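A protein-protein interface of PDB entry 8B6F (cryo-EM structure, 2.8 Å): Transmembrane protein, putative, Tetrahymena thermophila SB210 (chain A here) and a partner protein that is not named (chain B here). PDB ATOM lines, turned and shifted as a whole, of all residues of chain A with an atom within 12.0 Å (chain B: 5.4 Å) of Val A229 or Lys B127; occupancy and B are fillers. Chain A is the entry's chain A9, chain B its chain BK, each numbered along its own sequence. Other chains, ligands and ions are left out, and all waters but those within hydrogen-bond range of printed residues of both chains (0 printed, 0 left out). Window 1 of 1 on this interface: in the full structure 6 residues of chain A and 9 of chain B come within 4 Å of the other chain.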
ATOM      1  N   TYR A 220      30.638 -18.514 -21.438  1.00  0.00           N
ATOM      2  CA  TYR A 220      30.540 -17.125 -21.863  1.00  0.00           C
ATOM      3  C   TYR A 220      30.802 -16.190 -20.689  1.00  0.00           C
ATOM      4  O   TYR A 220      30.267 -16.382 -19.594  1.00  0.00           O
ATOM      5  CB  TYR A 220      29.159 -16.857 -22.460  1.00  0.00           C
ATOM      6  CG  TYR A 220      28.927 -17.573 -23.763  1.00  0.00           C
ATOM      7  CD1 TYR A 220      29.522 -17.130 -24.933  1.00  0.00           C
ATOM      8  CD2 TYR A 220      28.117 -18.696 -23.823  1.00  0.00           C
ATOM      9  CE1 TYR A 220      29.316 -17.783 -26.126  1.00  0.00           C
ATOM     10  CE2 TYR A 220      27.906 -19.357 -25.011  1.00  0.00           C
ATOM     11  CZ  TYR A 220      28.514 -18.899 -26.157  1.00  0.00           C
ATOM     12  OH  TYR A 220      28.304 -19.553 -27.344  1.00  0.00           O
ATOM     13  N   HIS A 221      31.620 -15.166 -20.927  1.00  0.00           N
ATOM     14  CA  HIS A 221      31.990 -14.255 -19.849  1.00  0.00           C
ATOM     15  C   HIS A 221      30.814 -13.382 -19.436  1.00  0.00           C
ATOM     16  O   HIS A 221      30.623 -13.111 -18.246  1.00  0.00           O
ATOM     17  CB  HIS A 221      33.176 -13.387 -20.270  1.00  0.00           C
ATOM     18  CG  HIS A 221      34.277 -14.149 -20.938  1.00  0.00           C
ATOM     19  ND1 HIS A 221      35.118 -13.576 -21.866  1.00  0.00           N
ATOM     20  CD2 HIS A 221      34.674 -15.436 -20.816  1.00  0.00           C
ATOM     21  CE1 HIS A 221      35.987 -14.477 -22.285  1.00  0.00           C
ATOM     22  NE2 HIS A 221      35.740 -15.615 -21.664  1.00  0.00           N
ATOM     23  N   LYS A 222      30.020 -12.926 -20.405  1.00  0.00           N
ATOM     24  CA  LYS A 222      28.924 -12.014 -20.097  1.00  0.00           C
ATOM     25  C   LYS A 222      27.893 -12.674 -19.189  1.00  0.00           C
ATOM     26  O   LYS A 222      27.430 -12.068 -18.216  1.00  0.00           O
ATOM     27  CB  LYS A 222      28.273 -11.530 -21.393  1.00  0.00           C
ATOM     28  CG  LYS A 222      29.155 -10.615 -22.228  1.00  0.00           C
ATOM     29  CD  LYS A 222      29.388  -9.281 -21.534  1.00  0.00           C
ATOM     30  CE  LYS A 222      30.125  -8.310 -22.441  1.00  0.00           C
ATOM     31  NZ  LYS A 222      30.333  -6.989 -21.787  1.00  0.00           N
ATOM     32  N   VAL A 223      27.512 -13.916 -19.491  1.00  0.00           N
ATOM     33  CA  VAL A 223      26.517 -14.592 -18.664  1.00  0.00           C
ATOM     34  C   VAL A 223      27.092 -14.911 -17.290  1.00  0.00           C
ATOM     35  O   VAL A 223      26.409 -14.763 -16.269  1.00  0.00           O
ATOM     36  CB  VAL A 223      25.996 -15.861 -19.367  1.00  0.00           C
ATOM     37  CG1 VAL A 223      25.454 -15.535 -20.744  1.00  0.00           C
ATOM     38  CG2 VAL A 223      27.069 -16.917 -19.453  1.00  0.00           C
ATOM     39  N   ARG A 224      28.351 -15.349 -17.235  1.00  0.00           N
ATOM     40  CA  ARG A 224      28.962 -15.668 -15.949  1.00  0.00           C
ATOM     41  C   ARG A 224      29.024 -14.440 -15.053  1.00  0.00           C
ATOM     42  O   ARG A 224      28.735 -14.521 -13.854  1.00  0.00           O
ATOM     43  CB  ARG A 224      30.362 -16.241 -16.156  1.00  0.00           C
ATOM     44  CG  ARG A 224      30.969 -16.828 -14.891  1.00  0.00           C
ATOM     45  CD  ARG A 224      32.446 -17.141 -15.056  1.00  0.00           C
ATOM     46  NE  ARG A 224      32.720 -17.794 -16.330  1.00  0.00           N
ATOM     47  CZ  ARG A 224      33.321 -17.223 -17.366  1.00  0.00           C
ATOM     48  NH1 ARG A 224      33.777 -15.982 -17.311  1.00  0.00           N
ATOM     49  NH2 ARG A 224      33.467 -17.917 -18.491  1.00  0.00           N
ATOM     50  N   ASN A 225      29.399 -13.294 -15.614  1.00  0.00           N
ATOM     51  CA  ASN A 225      29.511 -12.065 -14.843  1.00  0.00           C
ATOM     52  C   ASN A 225      28.188 -11.326 -14.710  1.00  0.00           C
ATOM     53  O   ASN A 225      28.134 -10.316 -14.003  1.00  0.00           O
ATOM     54  CB  ASN A 225      30.551 -11.141 -15.479  1.00  0.00           C
ATOM     55  CG  ASN A 225      31.899 -11.811 -15.648  1.00  0.00           C
ATOM     56  OD1 ASN A 225      32.449 -11.854 -16.747  1.00  0.00           O
ATOM     57  ND2 ASN A 225      32.436 -12.341 -14.557  1.00  0.00           N
ATOM     58  N   GLY A 226      27.127 -11.793 -15.359  1.00  0.00           N
ATOM     59  CA  GLY A 226      25.860 -11.085 -15.280  1.00  0.00           C
ATOM     60  C   GLY A 226      25.937  -9.681 -15.838  1.00  0.00           C
ATOM     61  O   GLY A 226      25.417  -8.741 -15.223  1.00  0.00           O
ATOM     62  N   GLN A 227      26.580  -9.516 -16.989  1.00  0.00           N
ATOM     63  CA  GLN A 227      26.786  -8.216 -17.616  1.00  0.00           C
ATOM     64  C   GLN A 227      26.066  -8.137 -18.955  1.00  0.00           C
ATOM     65  O   GLN A 227      26.599  -7.624 -19.941  1.00  0.00           O
ATOM     66  CB  GLN A 227      28.277  -7.937 -17.790  1.00  0.00           C
ATOM     67  CG  GLN A 227      29.043  -7.887 -16.477  1.00  0.00           C
ATOM     68  CD  GLN A 227      30.518  -7.597 -16.665  1.00  0.00           C
ATOM     69  OE1 GLN A 227      31.103  -6.807 -15.925  1.00  0.00           O
ATOM     70  NE2 GLN A 227      31.134  -8.245 -17.647  1.00  0.00           N
ATOM     71  N   LEU A 228      24.842  -8.654 -19.004  1.00  0.00           N
ATOM     72  CA  LEU A 228      24.020  -8.637 -20.204  1.00  0.00           C
ATOM     73  C   LEU A 228      22.867  -7.660 -20.034  1.00  0.00           C
ATOM     74  O   LEU A 228      22.247  -7.594 -18.968  1.00  0.00           O
ATOM     75  CB  LEU A 228      23.463 -10.029 -20.515  1.00  0.00           C
ATOM     76  CG  LEU A 228      24.433 -11.089 -21.033  1.00  0.00           C
ATOM     77  CD1 LEU A 228      23.700 -12.400 -21.211  1.00  0.00           C
ATOM     78  CD2 LEU A 228      25.081 -10.668 -22.338  1.00  0.00           C
ATOM     79  N   VAL A 229      22.583  -6.903 -21.095  1.00  0.00           N
ATOM     80  CA  VAL A 229      21.424  -6.021 -21.095  1.00  0.00           C
ATOM     81  C   VAL A 229      20.159  -6.855 -21.262  1.00  0.00           C
ATOM     82  O   VAL A 229      20.186  -7.965 -21.808  1.00  0.00           O
ATOM     83  CB  VAL A 229      21.557  -4.964 -22.208  1.00  0.00           C
ATOM     84  CG1 VAL A 229      20.328  -4.065 -22.269  1.00  0.00           C
ATOM     85  CG2 VAL A 229      22.809  -4.130 -21.999  1.00  0.00           C
ATOM     86  N   ASP A 230      19.040  -6.322 -20.780  1.00  0.00           N
ATOM     87  CA  ASP A 230      17.762  -7.019 -20.862  1.00  0.00           C
ATOM     88  C   ASP A 230      17.210  -6.870 -22.274  1.00  0.00           C
ATOM     89  O   ASP A 230      16.860  -5.765 -22.700  1.00  0.00           O
ATOM     90  CB  ASP A 230      16.785  -6.469 -19.829  1.00  0.00           C
ATOM     91  CG  ASP A 230      17.254  -6.700 -18.405  1.00  0.00           C
ATOM     92  OD1 ASP A 230      18.223  -6.036 -17.983  1.00  0.00           O
ATOM     93  OD2 ASP A 230      16.657  -7.549 -17.710  1.00  0.00           O
ATOM     94  N   LEU A 231      17.135  -7.980 -23.000  1.00  0.00           N
ATOM     95  CA  LEU A 231      16.633  -7.970 -24.367  1.00  0.00           C
ATOM     96  C   LEU A 231      15.108  -7.995 -24.381  1.00  0.00           C
ATOM     97  O   LEU A 231      14.472  -8.496 -23.454  1.00  0.00           O
ATOM     98  CB  LEU A 231      17.193  -9.165 -25.143  1.00  0.00           C
ATOM     99  CG  LEU A 231      16.630  -9.403 -26.547  1.00  0.00           C
ATOM    100  CD1 LEU A 231      16.806  -8.179 -27.422  1.00  0.00           C
ATOM    101  CD2 LEU A 231      17.298 -10.609 -27.179  1.00  0.00           C
ATOM    102  OXT LEU A 231      14.474  -7.512 -25.318  1.00  0.00           O
ATOM    103  N   ASN B 122      14.309  -1.057 -28.677  1.00  0.00           N
ATOM    104  CA  ASN B 122      14.670  -0.724 -27.303  1.00  0.00           C
ATOM    105  C   ASN B 122      16.006  -1.344 -26.916  1.00  0.00           C
ATOM    106  O   ASN B 122      16.837  -0.695 -26.271  1.00  0.00           O
ATOM    107  CB  ASN B 122      13.572  -1.190 -26.348  1.00  0.00           C
ATOM    108  CG  ASN B 122      12.272  -0.445 -26.547  1.00  0.00           C
ATOM    109  OD1 ASN B 122      12.266   0.723 -26.932  1.00  0.00           O
ATOM    110  ND2 ASN B 122      11.158  -1.117 -26.285  1.00  0.00           N
ATOM    111  N   TYR B 123      16.227  -2.605 -27.293  1.00  0.00           N
ATOM    112  CA  TYR B 123      17.475  -3.274 -26.943  1.00  0.00           C
ATOM    113  C   TYR B 123      18.674  -2.592 -27.591  1.00  0.00           C
ATOM    114  O   TYR B 123      19.703  -2.376 -26.938  1.00  0.00           O
ATOM    115  CB  TYR B 123      17.409  -4.743 -27.357  1.00  0.00           C
ATOM    116  CG  TYR B 123      18.750  -5.430 -27.356  1.00  0.00           C
ATOM    117  CD1 TYR B 123      19.330  -5.857 -26.170  1.00  0.00           C
ATOM    118  CD2 TYR B 123      19.432  -5.662 -28.541  1.00  0.00           C
ATOM    119  CE1 TYR B 123      20.552  -6.487 -26.164  1.00  0.00           C
ATOM    120  CE2 TYR B 123      20.653  -6.292 -28.544  1.00  0.00           C
ATOM    121  CZ  TYR B 123      21.206  -6.703 -27.353  1.00  0.00           C
ATOM    122  OH  TYR B 123      22.424  -7.331 -27.357  1.00  0.00           O
ATOM    123  N   ASN B 124      18.563  -2.243 -28.872  1.00  0.00           N
ATOM    124  CA  ASN B 124      19.670  -1.573 -29.547  1.00  0.00           C
ATOM    125  C   ASN B 124      19.932  -0.203 -28.941  1.00  0.00           C
ATOM    126  O   ASN B 124      21.089   0.201 -28.777  1.00  0.00           O
ATOM    127  CB  ASN B 124      19.383  -1.458 -31.042  1.00  0.00           C
ATOM    128  CG  ASN B 124      19.334  -2.807 -31.731  1.00  0.00           C
ATOM    129  OD1 ASN B 124      18.341  -3.159 -32.363  1.00  0.00           O
ATOM    130  ND2 ASN B 124      20.414  -3.569 -31.616  1.00  0.00           N
ATOM    131  N   ALA B 125      18.873   0.534 -28.607  1.00  0.00           N
ATOM    132  CA  ALA B 125      19.060   1.829 -27.963  1.00  0.00           C
ATOM    133  C   ALA B 125      19.776   1.676 -26.629  1.00  0.00           C
ATOM    134  O   ALA B 125      20.699   2.438 -26.320  1.00  0.00           O
ATOM    135  CB  ALA B 125      17.709   2.518 -27.769  1.00  0.00           C
ATOM    136  N   ALA B 126      19.363   0.698 -25.822  1.00  0.00           N
ATOM    137  CA  ALA B 126      20.008   0.484 -24.533  1.00  0.00           C
ATOM    138  C   ALA B 126      21.469   0.093 -24.708  1.00  0.00           C
ATOM    139  O   ALA B 126      22.339   0.554 -23.959  1.00  0.00           O
ATOM    140  CB  ALA B 126      19.259  -0.589 -23.744  1.00  0.00           C
ATOM    141  N   LYS B 127      21.759  -0.766 -25.689  1.00  0.00           N
ATOM    142  CA  LYS B 127      23.136  -1.194 -25.911  1.00  0.00           C
ATOM    143  C   LYS B 127      24.006  -0.036 -26.382  1.00  0.00           C
ATOM    144  O   LYS B 127      25.156   0.097 -25.950  1.00  0.00           O
ATOM    145  CB  LYS B 127      23.168  -2.338 -26.924  1.00  0.00           C
ATOM    146  CG  LYS B 127      24.348  -3.275 -26.749  1.00  0.00           C
ATOM    147  CD  LYS B 127      24.158  -4.193 -25.554  1.00  0.00           C
ATOM    148  CE  LYS B 127      25.369  -5.088 -25.355  1.00  0.00           C
ATOM    149  NZ  LYS B 127      25.193  -6.015 -24.203  1.00  0.00           N
ATOM    150  N   ASN B 128      23.483   0.807 -27.275  1.00  0.00           N
ATOM    151  CA  ASN B 128      24.242   1.969 -27.723  1.00  0.00           C
ATOM    152  C   ASN B 128      24.489   2.937 -26.575  1.00  0.00           C
ATOM    153  O   ASN B 128      25.567   3.532 -26.475  1.00  0.00           O
ATOM    154  CB  ASN B 128      23.511   2.665 -28.869  1.00  0.00           C
ATOM    155  CG  ASN B 128      23.455   1.817 -30.125  1.00  0.00           C
ATOM    156  OD1 ASN B 128      24.341   1.004 -30.378  1.00  0.00           O
ATOM    157  ND2 ASN B 128      22.411   2.007 -30.922  1.00  0.00           N
ATOM    158  N   LYS B 129      23.495   3.116 -25.701  1.00  0.00           N
ATOM    159  CA  LYS B 129      23.690   3.947 -24.518  1.00  0.00           C
ATOM    160  C   LYS B 129      24.757   3.357 -23.607  1.00  0.00           C
ATOM    161  O   LYS B 129      25.586   4.088 -23.054  1.00  0.00           O
ATOM    162  CB  LYS B 129      22.367   4.100 -23.765  1.00  0.00           C
ATOM    163  CG  LYS B 129      22.476   4.888 -22.467  1.00  0.00           C
ATOM    164  CD  LYS B 129      21.116   5.051 -21.804  1.00  0.00           C
ATOM    165  CE  LYS B 129      21.239   5.721 -20.445  1.00  0.00           C
ATOM    166  NZ  LYS B 129      21.873   7.067 -20.537  1.00  0.00           N
ATOM    167  N   GLU B 130      24.748   2.035 -23.435  1.00  0.00           N
ATOM    168  CA  GLU B 130      25.743   1.385 -22.592  1.00  0.00           C
ATOM    169  C   GLU B 130      27.146   1.522 -23.168  1.00  0.00           C
ATOM    170  O   GLU B 130      28.118   1.610 -22.410  1.00  0.00           O
ATOM    171  CB  GLU B 130      25.394  -0.093 -22.416  1.00  0.00           C
ATOM    172  CG  GLU B 130      26.383  -0.870 -21.553  1.00  0.00           C
ATOM    173  CD  GLU B 130      26.144  -2.367 -21.595  1.00  0.00           C
ATOM    174  OE1 GLU B 130      25.415  -2.829 -22.496  1.00  0.00           O
ATOM    175  OE2 GLU B 130      26.685  -3.081 -20.726  1.00  0.00           O
ATOM    176  N   ALA B 131      27.273   1.537 -24.495  1.00  0.00           N
ATOM    177  CA  ALA B 131      28.593   1.550 -25.112  1.00  0.00           C
ATOM    178  C   ALA B 131      29.421   2.751 -24.683  1.00  0.00           C
ATOM    179  O   ALA B 131      30.651   2.703 -24.771  1.00  0.00           O
ATOM    180  CB  ALA B 131      28.456   1.530 -26.633  1.00  0.00           C
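The side-chain amino group of Lys B127 lies within salt-bridge range of the side-chain carboxylate of Glu B130.
Among the printed residues, merely in contact across the chains: Val A229 with Ala B126, Val A229 with Lys B127, Val A229 with Glu B130 and Leu A231 with Tyr B123.
Asn A225 touches none of the printed residues of chain B. Gln A227 touches none of the printed residues of chain B. Of chain B, only Ala B126, Lys B127 and Glu B130 come within 4 Å of Val A229. Of the printed residues of chain B, Leu A231 touches Tyr B123. Tyr B123 touches just one residue of chain A: Leu A231 (3.4 Å). No residue of chain A comes within 4 Å of Ala B125. Of chain A, only Val A229 (3.9 Å) comes within 4 Å of Ala B126. Of chain A, only Val A229 (3.8 Å) comes within 4 Å of Lys B127. Printed residues of chain A within 4 Å of Glu B130: Val A229 (3.0 Å). No residue of chain A comes within 4 Å of Ala B131. The nearest residue of chain A that does not touch Lys B127 is Gln A227 (4.8 Å). The nearest printed residue of chain B that does not touch Leu A231 is Asn B124 (6.4 Å).
Of the 12 printed residues of chain A, 2 touch a printed residue of chain B. Printed residues of chain B that touch a printed residue of chain A: Tyr B123, Ala B126, Lys B127 and Glu B130. Among the printed residues, 4 pairs touch across the chains.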
